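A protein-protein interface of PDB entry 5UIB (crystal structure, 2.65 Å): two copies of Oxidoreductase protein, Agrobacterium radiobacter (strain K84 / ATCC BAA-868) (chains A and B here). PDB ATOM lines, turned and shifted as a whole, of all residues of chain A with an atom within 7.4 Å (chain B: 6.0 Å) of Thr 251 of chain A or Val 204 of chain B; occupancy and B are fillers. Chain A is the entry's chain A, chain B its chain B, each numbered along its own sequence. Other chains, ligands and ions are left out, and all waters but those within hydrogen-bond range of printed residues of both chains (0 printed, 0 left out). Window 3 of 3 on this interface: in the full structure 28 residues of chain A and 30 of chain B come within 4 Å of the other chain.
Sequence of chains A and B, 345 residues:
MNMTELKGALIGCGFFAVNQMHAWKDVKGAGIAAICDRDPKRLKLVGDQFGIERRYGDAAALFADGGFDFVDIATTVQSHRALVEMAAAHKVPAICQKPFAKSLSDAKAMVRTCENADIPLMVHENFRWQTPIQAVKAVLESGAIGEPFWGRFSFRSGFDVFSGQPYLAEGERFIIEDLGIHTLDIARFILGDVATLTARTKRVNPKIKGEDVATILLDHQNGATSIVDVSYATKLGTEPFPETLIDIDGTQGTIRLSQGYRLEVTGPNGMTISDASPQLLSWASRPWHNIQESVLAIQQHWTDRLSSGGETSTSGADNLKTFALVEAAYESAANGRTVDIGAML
NZ of Lys 202 of chain B lies within hydrogen-bond range of O of Phe 149 of chain A.
The backbone carbonyl oxygen (O) of Thr 251 of chain A lies within hydrogen-bond range of the side-chain amino group (NZ) of Lys 235 of chain B (3.0 Å).
The backbone carbonyl oxygen of Lys 235 of chain B lies within hydrogen-bond range of the side-chain hydroxyl of Thr 254 of chain A (2.7 Å).
N of Thr 251 of chain A lies within hydrogen-bond range of O of Glu 147 of chain A, at 3.1 Å.
N of Phe 149 of chain A sits at hydrogen-bond distance from O of Asp 249 of chain A, at 2.9 Å.
The backbone carbonyl oxygen (O) of Lys 202 of chain B sits at hydrogen-bond distance from the backbone NH (N) of Asp 212 of chain B, 3.3 Å away.
N of Lys 202 of chain B lies within hydrogen-bond range of O of Val 213 of chain B (3.2 Å).
The backbone NH (N) of Val 204 of chain B is in hydrogen-bond range of the side-chain carboxylate (OD1) of Asp 212 of chain B, 2.8 Å away.
Among the printed residues, pairs that only touch across the chains: Phe 149 of chain A with Ala 233 of chain B (3.3 Å), Phe 149 of chain A with Val 213 of chain B (3.7 Å), Thr 251 of chain A with Val 204 of chain B (3.7 Å) and Phe 149 of chain A with Val 204 of chain B (3.8 Å).
Pro 148 of chain A touches none of the printed residues of chain B.
Of chain B, only Val 204 and Lys 235 come within 4 Å of Thr 251 of chain A.
Of the printed residues of chain A, Lys 202 of chain B touches Phe 149.
Of chain A, only Phe 149 (3.8 Å) and Thr 251 (3.7 Å) come within 4 Å of Val 204 of chain B.
Asn 205 of chain B touches none of the printed residues of chain A.
Printed residues of chain A within 4 Å of Val 213 of chain B: Phe 149.
Printed residues of chain A within 4 Å of Ala 233 of chain B: Phe 149 (3.3 Å).
Printed residues of chain A within 4 Å of Lys 235 of chain B: Thr 251 and Thr 254.
The nearest printed residue of chain A that does not touch Ala 233 of chain B is Gly 250 of chain A (4.6 Å).
Of the 12 printed residues of chain A, 3 touch a printed residue of chain B.
Printed residues of chain A that touch a printed residue of chain B: Phe 149, Thr 251 and Thr 254.
Hydrophobic or aromatic side chains of chain A that line the printed part of chain B: Phe 149.
Of the 11 printed residues of chain B, 5 touch a printed residue of chain A.
Hydrophobic or aromatic side chains of chain B within 4 Å of the printed part of chain A: Val 204 and Val 213.
Among the printed residues, no Asp or Glu carboxylate lies within 4 Å of a Lys or Arg side-chain nitrogen of the other chain.
No position is printed for both chains.
Of the 7 pairs that touch across the chains among the printed residues, none has its exchanged pair printed and touching as well.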
ATOM      1  N   ILE A 145      26.738 -14.752  14.322  1.00  0.00           N
ATOM      2  CA  ILE A 145      27.273 -13.386  14.401  1.00  0.00           C
ATOM      3  C   ILE A 145      26.187 -12.319  14.576  1.00  0.00           C
ATOM      4  O   ILE A 145      26.445 -11.139  14.338  1.00  0.00           O
ATOM      5  CB  ILE A 145      28.129 -13.046  13.152  1.00  0.00           C
ATOM      6  CG1 ILE A 145      27.301 -13.085  11.854  1.00  0.00           C
ATOM      7  CG2 ILE A 145      29.309 -13.999  13.058  1.00  0.00           C
ATOM      8  CD1 ILE A 145      27.946 -12.373  10.680  1.00  0.00           C
ATOM      9  N   GLY A 146      24.984 -12.714  14.992  1.00  0.00           N
ATOM     10  CA  GLY A 146      23.886 -11.761  15.183  1.00  0.00           C
ATOM     11  C   GLY A 146      23.359 -11.135  13.903  1.00  0.00           C
ATOM     12  O   GLY A 146      23.663 -11.601  12.805  1.00  0.00           O
ATOM     13  N   GLU A 147      22.586 -10.060  14.054  1.00  0.00           N
ATOM     14  CA  GLU A 147      21.918  -9.404  12.923  1.00  0.00           C
ATOM     15  C   GLU A 147      22.990  -8.828  11.975  1.00  0.00           C
ATOM     16  O   GLU A 147      23.817  -8.030  12.417  1.00  0.00           O
ATOM     17  CB  GLU A 147      20.979  -8.277  13.408  1.00  0.00           C
ATOM     18  CG  GLU A 147      19.988  -8.645  14.508  1.00  0.00           C
ATOM     19  N   PRO A 148      23.014  -9.253  10.687  1.00  0.00           N
ATOM     20  CA  PRO A 148      24.036  -8.699   9.773  1.00  0.00           C
ATOM     21  C   PRO A 148      23.747  -7.241   9.397  1.00  0.00           C
ATOM     22  O   PRO A 148      22.610  -6.925   9.042  1.00  0.00           O
ATOM     23  CB  PRO A 148      23.959  -9.620   8.542  1.00  0.00           C
ATOM     24  CG  PRO A 148      22.606 -10.228   8.594  1.00  0.00           C
ATOM     25  CD  PRO A 148      22.203 -10.301  10.037  1.00  0.00           C
ATOM     26  N   PHE A 149      24.758  -6.371   9.507  1.00  0.00           N
ATOM     27  CA  PHE A 149      24.597  -4.932   9.221  1.00  0.00           C
ATOM     28  C   PHE A 149      25.438  -4.377   8.063  1.00  0.00           C
ATOM     29  O   PHE A 149      25.137  -3.298   7.556  1.00  0.00           O
ATOM     30  CB  PHE A 149      24.834  -4.103  10.490  1.00  0.00           C
ATOM     31  CG  PHE A 149      26.265  -4.069  10.956  1.00  0.00           C
ATOM     32  CD1 PHE A 149      27.191  -3.208  10.361  1.00  0.00           C
ATOM     33  CD2 PHE A 149      26.685  -4.872  12.010  1.00  0.00           C
ATOM     34  CE1 PHE A 149      28.510  -3.171  10.790  1.00  0.00           C
ATOM     35  CE2 PHE A 149      28.003  -4.830  12.451  1.00  0.00           C
ATOM     36  CZ  PHE A 149      28.915  -3.978  11.840  1.00  0.00           C
ATOM     37  N   TRP A 150      26.503  -5.070   7.675  1.00  0.00           N
ATOM     38  CA  TRP A 150      27.373  -4.590   6.610  1.00  0.00           C
ATOM     39  C   TRP A 150      27.982  -5.771   5.886  1.00  0.00           C
ATOM     40  O   TRP A 150      28.336  -6.762   6.519  1.00  0.00           O
ATOM     41  CB  TRP A 150      28.481  -3.686   7.181  1.00  0.00           C
ATOM     42  CG  TRP A 150      29.440  -3.164   6.140  1.00  0.00           C
ATOM     43  CD1 TRP A 150      29.314  -2.016   5.399  1.00  0.00           C
ATOM     44  CD2 TRP A 150      30.662  -3.784   5.716  1.00  0.00           C
ATOM     45  NE1 TRP A 150      30.383  -1.884   4.539  1.00  0.00           N
ATOM     46  CE2 TRP A 150      31.228  -2.951   4.713  1.00  0.00           C
ATOM     47  CE3 TRP A 150      31.338  -4.961   6.090  1.00  0.00           C
ATOM     48  CZ2 TRP A 150      32.447  -3.256   4.077  1.00  0.00           C
ATOM     49  CZ3 TRP A 150      32.552  -5.267   5.456  1.00  0.00           C
ATOM     50  CH2 TRP A 150      33.093  -4.412   4.461  1.00  0.00           C
ATOM     51  N   ASP A 249      29.747  -8.290   8.512  1.00  0.00           N
ATOM     52  CA  ASP A 249      29.791  -7.889   9.909  1.00  0.00           C
ATOM     53  C   ASP A 249      28.379  -7.912  10.472  1.00  0.00           C
ATOM     54  O   ASP A 249      27.440  -7.468   9.807  1.00  0.00           O
ATOM     55  CB  ASP A 249      30.361  -6.478  10.049  1.00  0.00           C
ATOM     56  CG  ASP A 249      31.806  -6.378   9.626  1.00  0.00           C
ATOM     57  OD1 ASP A 249      32.405  -7.400   9.222  1.00  0.00           O
ATOM     58  OD2 ASP A 249      32.343  -5.254   9.704  1.00  0.00           O
ATOM     59  N   GLY A 250      28.244  -8.428  11.694  1.00  0.00           N
ATOM     60  CA  GLY A 250      26.985  -8.387  12.436  1.00  0.00           C
ATOM     61  C   GLY A 250      27.177  -7.996  13.888  1.00  0.00           C
ATOM     62  O   GLY A 250      28.289  -8.039  14.405  1.00  0.00           O
ATOM     63  N   THR A 251      26.074  -7.657  14.551  1.00  0.00           N
ATOM     64  CA  THR A 251      26.087  -7.208  15.951  1.00  0.00           C
ATOM     65  C   THR A 251      26.850  -8.114  16.936  1.00  0.00           C
ATOM     66  O   THR A 251      27.429  -7.617  17.899  1.00  0.00           O
ATOM     67  CB  THR A 251      24.655  -7.039  16.493  1.00  0.00           C
ATOM     68  OG1 THR A 251      23.960  -8.294  16.417  1.00  0.00           O
ATOM     69  CG2 THR A 251      23.892  -5.972  15.702  1.00  0.00           C
ATOM     70  N   GLN A 252      26.838  -9.426  16.699  1.00  0.00           N
ATOM     71  CA  GLN A 252      27.551 -10.406  17.555  1.00  0.00           C
ATOM     72  C   GLN A 252      28.886 -10.951  16.985  1.00  0.00           C
ATOM     73  O   GLN A 252      29.573 -11.702  17.677  1.00  0.00           O
ATOM     74  CB  GLN A 252      26.613 -11.588  17.907  1.00  0.00           C
ATOM     75  CG  GLN A 252      25.986 -11.531  19.295  1.00  0.00           C
ATOM     76  CD  GLN A 252      25.345 -12.862  19.710  1.00  0.00           C
ATOM     77  OE1 GLN A 252      24.594 -13.486  18.947  1.00  0.00           O
ATOM     78  NE2 GLN A 252      25.637 -13.295  20.936  1.00  0.00           N
ATOM     79  N   GLY A 253      29.258 -10.592  15.754  1.00  0.00           N
ATOM     80  CA  GLY A 253      30.445 -11.178  15.123  1.00  0.00           C
ATOM     81  C   GLY A 253      30.716 -10.833  13.664  1.00  0.00           C
ATOM     82  O   GLY A 253      30.057  -9.970  13.084  1.00  0.00           O
ATOM     83  N   THR A 254      31.683 -11.539  13.074  1.00  0.00           N
ATOM     84  CA  THR A 254      32.144 -11.301  11.697  1.00  0.00           C
ATOM     85  C   THR A 254      32.404 -12.614  10.943  1.00  0.00           C
ATOM     86  O   THR A 254      32.884 -13.588  11.532  1.00  0.00           O
ATOM     87  CB  THR A 254      33.456 -10.467  11.663  1.00  0.00           C
ATOM     88  OG1 THR A 254      34.462 -11.099  12.465  1.00  0.00           O
ATOM     89  CG2 THR A 254      33.235  -9.030  12.178  1.00  0.00           C
ATOM     90  N   LYS B 202      25.189   4.042   9.724  1.00  0.00           N
ATOM     91  CA  LYS B 202      24.279   3.555  10.762  1.00  0.00           C
ATOM     92  C   LYS B 202      24.980   3.454  12.124  1.00  0.00           C
ATOM     93  O   LYS B 202      26.209   3.352  12.188  1.00  0.00           O
ATOM     94  CB  LYS B 202      23.720   2.189  10.373  1.00  0.00           C
ATOM     95  CG  LYS B 202      24.782   1.123  10.138  1.00  0.00           C
ATOM     96  CD  LYS B 202      24.206  -0.276  10.256  1.00  0.00           C
ATOM     97  CE  LYS B 202      23.101  -0.545   9.249  1.00  0.00           C
ATOM     98  NZ  LYS B 202      23.528  -0.243   7.853  1.00  0.00           N
ATOM     99  N   ARG B 203      24.192   3.484  13.200  1.00  0.00           N
ATOM    100  CA  ARG B 203      24.699   3.248  14.549  1.00  0.00           C
ATOM    101  C   ARG B 203      24.299   1.852  14.978  1.00  0.00           C
ATOM    102  O   ARG B 203      23.104   1.543  15.020  1.00  0.00           O
ATOM    103  CB  ARG B 203      24.140   4.264  15.544  1.00  0.00           C
ATOM    104  CG  ARG B 203      24.632   4.076  16.980  1.00  0.00           C
ATOM    105  CD  ARG B 203      24.166   5.212  17.876  1.00  0.00           C
ATOM    106  NE  ARG B 203      22.732   5.126  18.147  1.00  0.00           N
ATOM    107  CZ  ARG B 203      22.160   4.354  19.076  1.00  0.00           C
ATOM    108  NH1 ARG B 203      22.886   3.575  19.877  1.00  0.00           N
ATOM    109  NH2 ARG B 203      20.835   4.361  19.208  1.00  0.00           N
ATOM    110  N   VAL B 204      25.295   1.023  15.297  1.00  0.00           N
ATOM    111  CA  VAL B 204      25.069  -0.346  15.774  1.00  0.00           C
ATOM    112  C   VAL B 204      25.221  -0.446  17.292  1.00  0.00           C
ATOM    113  O   VAL B 204      24.364  -1.026  17.959  1.00  0.00           O
ATOM    114  CB  VAL B 204      26.014  -1.350  15.080  1.00  0.00           C
ATOM    115  CG1 VAL B 204      25.798  -2.770  15.610  1.00  0.00           C
ATOM    116  CG2 VAL B 204      25.798  -1.304  13.572  1.00  0.00           C
ATOM    117  N   ASN B 205      26.312   0.091  17.829  1.00  0.00           N
ATOM    118  CA  ASN B 205      26.542   0.071  19.270  1.00  0.00           C
ATOM    119  C   ASN B 205      25.355   0.753  19.964  1.00  0.00           C
ATOM    120  O   ASN B 205      25.052   1.909  19.651  1.00  0.00           O
ATOM    121  CB  ASN B 205      27.863   0.786  19.610  1.00  0.00           C
ATOM    122  CG  ASN B 205      28.261   0.670  21.081  1.00  0.00           C
ATOM    123  OD1 ASN B 205      27.539   0.103  21.906  1.00  0.00           O
ATOM    124  ND2 ASN B 205      29.428   1.218  21.411  1.00  0.00           N
ATOM    125  N   PRO B 206      24.663   0.037  20.884  1.00  0.00           N
ATOM    126  CA  PRO B 206      23.562   0.686  21.620  1.00  0.00           C
ATOM    127  C   PRO B 206      23.988   1.813  22.578  1.00  0.00           C
ATOM    128  O   PRO B 206      23.175   2.691  22.872  1.00  0.00           O
ATOM    129  CB  PRO B 206      22.917  -0.472  22.403  1.00  0.00           C
ATOM    130  CG  PRO B 206      23.960  -1.530  22.475  1.00  0.00           C
ATOM    131  CD  PRO B 206      24.750  -1.403  21.205  1.00  0.00           C
ATOM    132  N   LYS B 207      25.240   1.800  23.034  1.00  0.00           N
ATOM    133  CA  LYS B 207      25.699   2.698  24.101  1.00  0.00           C
ATOM    134  C   LYS B 207      25.984   4.144  23.683  1.00  0.00           C
ATOM    135  O   LYS B 207      25.816   5.059  24.490  1.00  0.00           O
ATOM    136  CB  LYS B 207      26.941   2.113  24.768  1.00  0.00           C
ATOM    137  CG  LYS B 207      26.681   0.766  25.414  1.00  0.00           C
ATOM    138  CD  LYS B 207      27.950   0.177  25.977  1.00  0.00           C
ATOM    139  CE  LYS B 207      27.684  -1.217  26.493  1.00  0.00           C
ATOM    140  NZ  LYS B 207      28.826  -1.683  27.317  1.00  0.00           N
ATOM    141  N   GLY B 210      26.191   8.455  18.335  1.00  0.00           N
ATOM    142  CA  GLY B 210      26.550   8.704  16.925  1.00  0.00           C
ATOM    143  C   GLY B 210      26.697   7.472  16.046  1.00  0.00           C
ATOM    144  O   GLY B 210      26.741   6.344  16.536  1.00  0.00           O
ATOM    145  N   ASP B 212      28.488   4.741  14.057  1.00  0.00           N
ATOM    146  CA  ASP B 212      29.782   4.072  14.235  1.00  0.00           C
ATOM    147  C   ASP B 212      30.135   3.138  13.080  1.00  0.00           C
ATOM    148  O   ASP B 212      31.074   2.363  13.193  1.00  0.00           O
ATOM    149  CB  ASP B 212      29.862   3.340  15.588  1.00  0.00           C
ATOM    150  CG  ASP B 212      28.762   2.300  15.784  1.00  0.00           C
ATOM    151  OD1 ASP B 212      27.801   2.242  14.985  1.00  0.00           O
ATOM    152  OD2 ASP B 212      28.854   1.531  16.763  1.00  0.00           O
ATOM    153  N   VAL B 213      29.381   3.209  11.985  1.00  0.00           N
ATOM    154  CA  VAL B 213      29.712   2.497  10.758  1.00  0.00           C
ATOM    155  C   VAL B 213      29.430   3.434   9.598  1.00  0.00           C
ATOM    156  O   VAL B 213      28.345   4.014   9.533  1.00  0.00           O
ATOM    157  CB  VAL B 213      28.873   1.226  10.588  1.00  0.00           C
ATOM    158  CG1 VAL B 213      29.236   0.525   9.284  1.00  0.00           C
ATOM    159  CG2 VAL B 213      29.069   0.300  11.778  1.00  0.00           C
ATOM    160  N   ALA B 233      32.093  -0.983  15.273  1.00  0.00           N
ATOM    161  CA  ALA B 233      31.223  -2.072  15.738  1.00  0.00           C
ATOM    162  C   ALA B 233      31.542  -3.369  14.992  1.00  0.00           C
ATOM    163  O   ALA B 233      30.639  -4.099  14.617  1.00  0.00           O
ATOM    164  CB  ALA B 233      29.765  -1.695  15.534  1.00  0.00           C
ATOM    165  N   LYS B 235      33.704  -6.943  15.135  1.00  0.00           N
ATOM    166  CA  LYS B 235      34.310  -7.866  16.081  1.00  0.00           C
ATOM    167  C   LYS B 235      35.112  -8.958  15.375  1.00  0.00           C
ATOM    168  O   LYS B 235      34.568  -9.967  14.941  1.00  0.00           O
ATOM    169  CB  LYS B 235      33.215  -8.444  16.973  1.00  0.00           C
ATOM    170  CG  LYS B 235      32.310  -7.352  17.545  1.00  0.00           C
ATOM    171  CD  LYS B 235      31.737  -7.715  18.906  1.00  0.00           C
ATOM    172  CE  LYS B 235      31.144  -6.511  19.628  1.00  0.00           C
ATOM    173  NZ  LYS B 235      29.752  -6.253  19.177  1.00  0.00           N
